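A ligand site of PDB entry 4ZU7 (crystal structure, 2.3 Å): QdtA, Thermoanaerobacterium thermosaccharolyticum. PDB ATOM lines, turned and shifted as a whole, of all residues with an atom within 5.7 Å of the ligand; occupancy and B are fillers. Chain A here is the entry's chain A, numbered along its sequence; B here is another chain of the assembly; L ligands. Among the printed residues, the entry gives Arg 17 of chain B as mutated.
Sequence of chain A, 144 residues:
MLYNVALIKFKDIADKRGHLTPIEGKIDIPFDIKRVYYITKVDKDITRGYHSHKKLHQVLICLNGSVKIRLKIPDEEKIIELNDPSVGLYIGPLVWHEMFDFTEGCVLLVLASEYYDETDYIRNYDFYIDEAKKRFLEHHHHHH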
ATOM      1  N   ARG A  35     -33.241   9.111 -28.475  1.00  0.00           N
ATOM      2  CA  ARG A  35     -33.626  10.506 -28.497  1.00  0.00           C
ATOM      3  C   ARG A  35     -32.942  11.184 -29.647  1.00  0.00           C
ATOM      4  O   ARG A  35     -31.784  10.835 -29.965  1.00  0.00           O
ATOM      5  CB  ARG A  35     -33.141  11.175 -27.235  1.00  0.00           C
ATOM      6  CG  ARG A  35     -33.168  12.682 -27.301  1.00  0.00           C
ATOM      7  CD  ARG A  35     -32.960  13.244 -25.891  1.00  0.00           C
ATOM      8  NE  ARG A  35     -31.670  12.813 -25.309  1.00  0.00           N
ATOM      9  CZ  ARG A  35     -30.684  13.651 -25.030  1.00  0.00           C
ATOM     10  NH1 ARG A  35     -29.575  13.179 -24.524  1.00  0.00           N
ATOM     11  NH2 ARG A  35     -30.808  14.971 -25.263  1.00  0.00           N
ATOM     12  N   VAL A  36     -33.660  12.092 -30.316  1.00  0.00           N
ATOM     13  CA  VAL A  36     -33.022  13.027 -31.226  1.00  0.00           C
ATOM     14  C   VAL A  36     -33.290  14.452 -30.805  1.00  0.00           C
ATOM     15  O   VAL A  36     -34.232  14.724 -30.064  1.00  0.00           O
ATOM     16  CB  VAL A  36     -33.406  12.869 -32.712  1.00  0.00           C
ATOM     17  CG1 VAL A  36     -33.284  11.431 -33.139  1.00  0.00           C
ATOM     18  CG2 VAL A  36     -34.805  13.373 -32.980  1.00  0.00           C
ATOM     19  N   TYR A  37     -32.444  15.355 -31.299  1.00  0.00           N
ATOM     20  CA  TYR A  37     -32.724  16.765 -31.206  1.00  0.00           C
ATOM     21  C   TYR A  37     -31.942  17.593 -32.224  1.00  0.00           C
ATOM     22  O   TYR A  37     -30.851  17.233 -32.671  1.00  0.00           O
ATOM     23  CB  TYR A  37     -32.535  17.312 -29.781  1.00  0.00           C
ATOM     24  CG  TYR A  37     -31.123  17.486 -29.345  1.00  0.00           C
ATOM     25  CD1 TYR A  37     -30.443  18.709 -29.553  1.00  0.00           C
ATOM     26  CD2 TYR A  37     -30.455  16.462 -28.730  1.00  0.00           C
ATOM     27  CE1 TYR A  37     -29.103  18.847 -29.161  1.00  0.00           C
ATOM     28  CE2 TYR A  37     -29.127  16.603 -28.350  1.00  0.00           C
ATOM     29  CZ  TYR A  37     -28.469  17.783 -28.546  1.00  0.00           C
ATOM     30  OH  TYR A  37     -27.171  17.850 -28.130  1.00  0.00           O
ATOM     31  N   ILE A  39     -31.086  21.756 -33.643  1.00  0.00           N
ATOM     32  CA  ILE A  39     -30.888  23.157 -33.395  1.00  0.00           C
ATOM     33  C   ILE A  39     -30.993  23.929 -34.711  1.00  0.00           C
ATOM     34  O   ILE A  39     -30.418  23.511 -35.710  1.00  0.00           O
ATOM     35  CB  ILE A  39     -29.516  23.317 -32.787  1.00  0.00           C
ATOM     36  CG1 ILE A  39     -29.554  22.653 -31.413  1.00  0.00           C
ATOM     37  CG2 ILE A  39     -29.108  24.785 -32.754  1.00  0.00           C
ATOM     38  CD1 ILE A  39     -28.255  22.705 -30.658  1.00  0.00           C
ATOM     39  N   ARG A  48     -22.681  27.850 -29.009  1.00  0.00           N
ATOM     40  CA  ARG A  48     -23.517  26.995 -28.160  1.00  0.00           C
ATOM     41  C   ARG A  48     -22.704  25.788 -27.724  1.00  0.00           C
ATOM     42  O   ARG A  48     -21.646  25.520 -28.281  1.00  0.00           O
ATOM     43  CB  ARG A  48     -24.676  26.404 -28.971  1.00  0.00           C
ATOM     44  CG  ARG A  48     -25.769  27.378 -29.332  1.00  0.00           C
ATOM     45  CD  ARG A  48     -26.988  26.667 -29.926  1.00  0.00           C
ATOM     46  NE  ARG A  48     -27.767  25.936 -28.929  1.00  0.00           N
ATOM     47  CZ  ARG A  48     -29.023  26.224 -28.567  1.00  0.00           C
ATOM     48  NH1 ARG A  48     -29.632  25.464 -27.691  1.00  0.00           N
ATOM     49  NH2 ARG A  48     -29.681  27.261 -29.080  1.00  0.00           N
ATOM     50  N   GLY A  49     -23.262  25.021 -26.793  1.00  0.00           N
ATOM     51  CA  GLY A  49     -22.605  23.802 -26.259  1.00  0.00           C
ATOM     52  C   GLY A  49     -22.003  24.042 -24.899  1.00  0.00           C
ATOM     53  O   GLY A  49     -22.704  24.385 -23.941  1.00  0.00           O
ATOM     54  N   TYR A  50     -20.691  23.888 -24.805  1.00  0.00           N
ATOM     55  CA  TYR A  50     -19.979  24.134 -23.566  1.00  0.00           C
ATOM     56  C   TYR A  50     -20.397  23.100 -22.536  1.00  0.00           C
ATOM     57  O   TYR A  50     -20.865  23.425 -21.469  1.00  0.00           O
ATOM     58  CB  TYR A  50     -20.226  25.547 -22.976  1.00  0.00           C
ATOM     59  CG  TYR A  50     -19.758  26.702 -23.791  1.00  0.00           C
ATOM     60  CD1 TYR A  50     -18.388  26.996 -23.902  1.00  0.00           C
ATOM     61  CD2 TYR A  50     -20.693  27.566 -24.400  1.00  0.00           C
ATOM     62  CE1 TYR A  50     -17.974  28.105 -24.606  1.00  0.00           C
ATOM     63  CE2 TYR A  50     -20.290  28.661 -25.105  1.00  0.00           C
ATOM     64  CZ  TYR A  50     -18.931  28.927 -25.204  1.00  0.00           C
ATOM     65  OH  TYR A  50     -18.551  30.042 -25.879  1.00  0.00           O
ATOM     66  N   HIS A  51     -20.205  21.837 -22.880  1.00  0.00           N
ATOM     67  CA  HIS A  51     -20.483  20.769 -21.961  1.00  0.00           C
ATOM     68  C   HIS A  51     -19.835  19.465 -22.363  1.00  0.00           C
ATOM     69  O   HIS A  51     -19.217  19.339 -23.474  1.00  0.00           O
ATOM     70  CB  HIS A  51     -22.012  20.608 -21.719  1.00  0.00           C
ATOM     71  CG  HIS A  51     -22.838  20.438 -22.948  1.00  0.00           C
ATOM     72  ND1 HIS A  51     -22.639  19.406 -23.845  1.00  0.00           N
ATOM     73  CD2 HIS A  51     -23.892  21.137 -23.419  1.00  0.00           C
ATOM     74  CE1 HIS A  51     -23.530  19.492 -24.816  1.00  0.00           C
ATOM     75  NE2 HIS A  51     -24.311  20.524 -24.574  1.00  0.00           N
ATOM     76  N   MET A  99     -20.107  24.550 -30.275  1.00  0.00           N
ATOM     77  CA  MET A  99     -20.533  24.707 -31.680  1.00  0.00           C
ATOM     78  C   MET A  99     -20.657  26.174 -32.034  1.00  0.00           C
ATOM     79  O   MET A  99     -21.344  26.935 -31.337  1.00  0.00           O
ATOM     80  CB  MET A  99     -21.897  24.063 -31.933  1.00  0.00           C
ATOM     81  CG  MET A  99     -22.057  22.619 -31.474  1.00  0.00           C
ATOM     82  SD  MET A  99     -22.971  22.483 -29.933  1.00  0.00           S
ATOM     83  CE  MET A  99     -24.643  22.290 -30.494  1.00  0.00           C
ATOM     84  N   TYR A 116     -32.819  12.406 -22.294  1.00  0.00           N
ATOM     85  CA  TYR A 116     -32.201  13.610 -21.687  1.00  0.00           C
ATOM     86  C   TYR A 116     -32.088  13.520 -20.180  1.00  0.00           C
ATOM     87  O   TYR A 116     -33.053  13.243 -19.497  1.00  0.00           O
ATOM     88  CB  TYR A 116     -33.019  14.865 -22.056  1.00  0.00           C
ATOM     89  CG  TYR A 116     -32.615  16.105 -21.297  1.00  0.00           C
ATOM     90  CD1 TYR A 116     -31.486  16.815 -21.668  1.00  0.00           C
ATOM     91  CD2 TYR A 116     -33.310  16.509 -20.170  1.00  0.00           C
ATOM     92  CE1 TYR A 116     -31.081  17.933 -20.958  1.00  0.00           C
ATOM     93  CE2 TYR A 116     -32.903  17.602 -19.442  1.00  0.00           C
ATOM     94  CZ  TYR A 116     -31.801  18.321 -19.851  1.00  0.00           C
ATOM     95  OH  TYR A 116     -31.411  19.422 -19.163  1.00  0.00           O
ATOM     96  N   GLU A 118     -30.151  15.570 -17.038  1.00  0.00           N
ATOM     97  CA  GLU A 118     -29.364  16.737 -16.649  1.00  0.00           C
ATOM     98  C   GLU A 118     -28.177  16.323 -15.812  1.00  0.00           C
ATOM     99  O   GLU A 118     -27.129  16.886 -15.954  1.00  0.00           O
ATOM    100  CB  GLU A 118     -30.199  17.801 -15.948  1.00  0.00           C
ATOM    101  CG  GLU A 118     -29.432  19.024 -15.531  1.00  0.00           C
ATOM    102  CD  GLU A 118     -28.647  19.736 -16.642  1.00  0.00           C
ATOM    103  OE1 GLU A 118     -27.463  20.093 -16.362  1.00  0.00           O
ATOM    104  OE2 GLU A 118     -29.224  19.996 -17.757  1.00  0.00           O
ATOM    105  N   TYR A 121     -24.788  15.582 -17.773  1.00  0.00           N
ATOM    106  CA  TYR A 121     -23.975  16.717 -18.215  1.00  0.00           C
ATOM    107  C   TYR A 121     -22.944  17.141 -17.198  1.00  0.00           C
ATOM    108  O   TYR A 121     -23.222  17.149 -16.021  1.00  0.00           O
ATOM    109  CB  TYR A 121     -24.832  17.980 -18.416  1.00  0.00           C
ATOM    110  CG  TYR A 121     -25.683  18.037 -19.654  1.00  0.00           C
ATOM    111  CD1 TYR A 121     -26.888  17.375 -19.705  1.00  0.00           C
ATOM    112  CD2 TYR A 121     -25.342  18.818 -20.719  1.00  0.00           C
ATOM    113  CE1 TYR A 121     -27.708  17.478 -20.795  1.00  0.00           C
ATOM    114  CE2 TYR A 121     -26.146  18.900 -21.823  1.00  0.00           C
ATOM    115  CZ  TYR A 121     -27.328  18.226 -21.858  1.00  0.00           C
ATOM    116  OH  TYR A 121     -28.144  18.273 -22.958  1.00  0.00           O
ATOM    117  N   ARG A 123     -21.223  20.780 -16.949  1.00  0.00           N
ATOM    118  CA  ARG A 123     -21.325  22.132 -17.515  1.00  0.00           C
ATOM    119  C   ARG A 123     -20.293  23.110 -16.996  1.00  0.00           C
ATOM    120  O   ARG A 123     -20.129  24.196 -17.558  1.00  0.00           O
ATOM    121  CB  ARG A 123     -22.721  22.734 -17.323  1.00  0.00           C
ATOM    122  CG  ARG A 123     -23.815  21.910 -18.017  1.00  0.00           C
ATOM    123  CD  ARG A 123     -25.209  22.417 -17.718  1.00  0.00           C
ATOM    124  NE  ARG A 123     -26.273  21.666 -18.397  1.00  0.00           N
ATOM    125  CZ  ARG A 123     -26.653  21.844 -19.676  1.00  0.00           C
ATOM    126  NH1 ARG A 123     -26.067  22.731 -20.512  1.00  0.00           N
ATOM    127  NH2 ARG A 123     -27.635  21.088 -20.131  1.00  0.00           N
ATOM    128  N   LYS B  11     -41.714  20.490 -28.040  1.00  0.00           N
ATOM    129  CA  LYS B  11     -41.002  21.565 -27.361  1.00  0.00           C
ATOM    130  C   LYS B  11     -40.070  22.325 -28.316  1.00  0.00           C
ATOM    131  O   LYS B  11     -39.302  21.730 -29.080  1.00  0.00           O
ATOM    132  CB  LYS B  11     -40.154  21.026 -26.210  1.00  0.00           C
ATOM    133  CG  LYS B  11     -40.942  20.287 -25.154  1.00  0.00           C
ATOM    134  CD  LYS B  11     -40.055  19.646 -24.077  1.00  0.00           C
ATOM    135  CE  LYS B  11     -40.714  18.400 -23.477  1.00  0.00           C
ATOM    136  NZ  LYS B  11     -39.837  17.193 -23.575  1.00  0.00           N
ATOM    137  N   ILE B  13     -37.451  25.117 -27.498  1.00  0.00           N
ATOM    138  CA  ILE B  13     -36.723  25.846 -26.480  1.00  0.00           C
ATOM    139  C   ILE B  13     -35.991  26.912 -27.268  1.00  0.00           C
ATOM    140  O   ILE B  13     -34.995  26.607 -27.922  1.00  0.00           O
ATOM    141  CB  ILE B  13     -35.787  24.911 -25.729  1.00  0.00           C
ATOM    142  CG1 ILE B  13     -36.614  24.069 -24.778  1.00  0.00           C
ATOM    143  CG2 ILE B  13     -34.739  25.657 -24.917  1.00  0.00           C
ATOM    144  CD1 ILE B  13     -36.149  22.627 -24.742  1.00  0.00           C
ATOM    145  N   ARG B  17     -29.875  32.191 -28.158  1.00  0.00           N
ATOM    146  CA  ARG B  17     -28.913  31.269 -28.792  1.00  0.00           C
ATOM    147  C   ARG B  17     -29.547  30.445 -29.916  1.00  0.00           C
ATOM    148  O   ARG B  17     -28.845  29.763 -30.675  1.00  0.00           O
ATOM    149  CB  ARG B  17     -28.338  30.319 -27.777  1.00  0.00           C
ATOM    150  CG  ARG B  17     -27.667  30.973 -26.601  1.00  0.00           C
ATOM    151  CD  ARG B  17     -28.059  30.233 -25.338  1.00  0.00           C
ATOM    152  NE  ARG B  17     -27.295  29.028 -25.169  1.00  0.00           N
ATOM    153  CZ  ARG B  17     -27.746  27.790 -24.931  1.00  0.00           C
ATOM    154  NH1 ARG B  17     -29.057  27.499 -24.837  1.00  0.00           N
ATOM    155  NH2 ARG B  17     -26.847  26.819 -24.791  1.00  0.00           N
ATOM    156  N   LEU B  20     -34.191  24.872 -30.299  1.00  0.00           N
ATOM    157  CA  LEU B  20     -33.818  23.499 -30.075  1.00  0.00           C
ATOM    158  C   LEU B  20     -35.103  22.772 -29.818  1.00  0.00           C
ATOM    159  O   LEU B  20     -35.887  23.172 -28.945  1.00  0.00           O
ATOM    160  CB  LEU B  20     -32.887  23.374 -28.870  1.00  0.00           C
ATOM    161  CG  LEU B  20     -32.323  21.965 -28.591  1.00  0.00           C
ATOM    162  CD1 LEU B  20     -30.944  22.059 -27.973  1.00  0.00           C
ATOM    163  CD2 LEU B  20     -33.204  21.148 -27.670  1.00  0.00           C
ATOM    164  N   PRO B  22     -36.258  18.834 -28.884  1.00  0.00           N
ATOM    165  CA  PRO B  22     -35.908  17.456 -28.512  1.00  0.00           C
ATOM    166  C   PRO B  22     -37.085  16.505 -28.724  1.00  0.00           C
ATOM    167  O   PRO B  22     -38.239  16.899 -28.515  1.00  0.00           O
ATOM    168  CB  PRO B  22     -35.621  17.575 -27.037  1.00  0.00           C
ATOM    169  CG  PRO B  22     -36.569  18.655 -26.561  1.00  0.00           C
ATOM    170  CD  PRO B  22     -36.733  19.620 -27.726  1.00  0.00           C
ATOM    171  N   ILE B  23     -36.793  15.264 -29.148  1.00  0.00           N
ATOM    172  CA  ILE B  23     -37.813  14.203 -29.356  1.00  0.00           C
ATOM    173  C   ILE B  23     -37.270  12.899 -28.743  1.00  0.00           C
ATOM    174  O   ILE B  23     -36.201  12.398 -29.144  1.00  0.00           O
ATOM    175  CB  ILE B  23     -38.102  14.002 -30.858  1.00  0.00           C
ATOM    176  CG1 ILE B  23     -38.451  15.323 -31.532  1.00  0.00           C
ATOM    177  CG2 ILE B  23     -39.239  13.040 -31.073  1.00  0.00           C
ATOM    178  CD1 ILE B  23     -38.687  15.244 -33.023  1.00  0.00           C
ATOM    179  N   GLU B  24     -37.979  12.374 -27.738  1.00  0.00           N
ATOM    180  CA  GLU B  24     -37.592  11.104 -27.099  1.00  0.00           C
ATOM    181  C   GLU B  24     -38.551  10.047 -27.579  1.00  0.00           C
ATOM    182  O   GLU B  24     -39.775  10.237 -27.544  1.00  0.00           O
ATOM    183  CB  GLU B  24     -37.612  11.236 -25.583  1.00  0.00           C
ATOM    184  CG  GLU B  24     -36.668  12.327 -25.088  1.00  0.00           C
ATOM    185  CD  GLU B  24     -36.679  12.513 -23.600  1.00  0.00           C
ATOM    186  OE1 GLU B  24     -37.771  12.504 -22.996  1.00  0.00           O
ATOM    187  OE2 GLU B  24     -35.579  12.679 -23.031  1.00  0.00           O
HETATM  188  P1  LIG L   1     -28.264  22.938 -23.810  1.00  0.00           P
HETATM  189  O1  LIG L   1     -27.899  23.902 -22.711  1.00  0.00           O
HETATM  190  O2  LIG L   1     -27.871  21.465 -23.657  1.00  0.00           O
HETATM  191  O3  LIG L   1     -27.871  23.559 -25.289  1.00  0.00           O
HETATM  192  P2  LIG L   1     -26.722  23.313 -26.455  1.00  0.00           P
HETATM  193  O4  LIG L   1     -25.674  24.311 -26.080  1.00  0.00           O
HETATM  194  O5  LIG L   1     -26.309  21.828 -26.627  1.00  0.00           O
HETATM  195  O6  LIG L   1     -27.416  23.790 -27.687  1.00  0.00           O
HETATM  196  O7  LIG L   1     -29.882  22.990 -23.969  1.00  0.00           O
HETATM  197  C1  LIG L   1     -30.762  24.067 -23.622  1.00  0.00           C
HETATM  198  C2  LIG L   1     -32.016  23.579 -22.865  1.00  0.00           C
HETATM  199  O8  LIG L   1     -32.758  22.637 -23.647  1.00  0.00           O
HETATM  200  C3  LIG L   1     -31.762  22.916 -21.513  1.00  0.00           C
HETATM  201  O9  LIG L   1     -32.599  23.420 -20.476  1.00  0.00           O
HETATM  202  C4  LIG L   1     -32.170  21.472 -21.666  1.00  0.00           C
HETATM  203  C5  LIG L   1     -33.151  21.525 -22.831  1.00  0.00           C
HETATM  204  N1  LIG L   1     -33.066  20.238 -23.524  1.00  0.00           N
HETATM  205  C6  LIG L   1     -34.103  19.268 -23.364  1.00  0.00           C
HETATM  206  O10 LIG L   1     -35.152  19.458 -22.676  1.00  0.00           O
HETATM  207  N2  LIG L   1     -33.990  18.101 -24.013  1.00  0.00           N
HETATM  208  C7  LIG L   1     -32.911  17.802 -24.768  1.00  0.00           C
HETATM  209  O11 LIG L   1     -32.874  16.691 -25.300  1.00  0.00           O
HETATM  210  C8  LIG L   1     -31.818  18.807 -24.917  1.00  0.00           C
HETATM  211  C9  LIG L   1     -30.582  18.573 -25.733  1.00  0.00           C
HETATM  212  C10 LIG L   1     -31.957  19.997 -24.253  1.00  0.00           C
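O4 of the ligand is in salt-bridge range of NH2 of Arg 17 of chain B (3.1 Å).
The side-chain hydroxyl of Tyr 121 lies within hydrogen-bond range of an oxygen (O2) of the ligand (3.3 Å).
The guanidinium group of Arg 48 lies within salt-bridge range of an oxygen (O6) of the ligand (2.5 Å).
NH2 of Arg 35 sits at hydrogen-bond distance from O11 of the ligand (2.7 Å).
NH1 of Arg 123 lies within salt-bridge range of O1 of the ligand, 3.1 Å away.
A ring nitrogen (NE2) of His 51 sits at hydrogen-bond distance from an oxygen (O5) of the ligand (3.1 Å).
N of Gly 49 is in hydrogen-bond range of O4 of the ligand (2.6 Å).
The side-chain carboxylate (OE2) of Glu 118 lies within hydrogen-bond range of the side-chain hydroxyl (OH) of Tyr 116, 2.7 Å away.
N of Tyr 116 sits at hydrogen-bond distance from OE2 of Glu 24 of chain B, 2.9 Å away.
N of Ile 13 of chain B sits at hydrogen-bond distance from O of Leu 20 of chain B (2.9 Å).
The guanidinium group (NH2) of Arg 48 is in hydrogen-bond range of the backbone carbonyl oxygen (O) of Arg 17 of chain B (3.1 Å).
OE1 of Glu 118 lies within salt-bridge range of NE of Arg 123.
The backbone carbonyl oxygen (O) of Arg 48 sits at hydrogen-bond distance from the backbone NH (N) of Met 99 (2.7 Å).
CE2 of Tyr 37 touches C9 of the ligand, at 3.6 Å.
Ile 39 touches the ligand (CD1 to O6, 3.3 Å).
Tyr 116 touches the ligand.
Ile 13 of chain B touches the ligand.
Leu 20 of chain B touches the ligand (CD2 to C10, 3.8 Å).
CB of Pro 22 of chain B touches O11 of the ligand (3.4 Å).
Hydrophobic or aromatic side chains that line the ligand: Tyr 37, Ile 39, His 51, Tyr 116, Tyr 121, Ile 13 of chain B, Leu 20 of chain B and Pro 22 of chain B.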
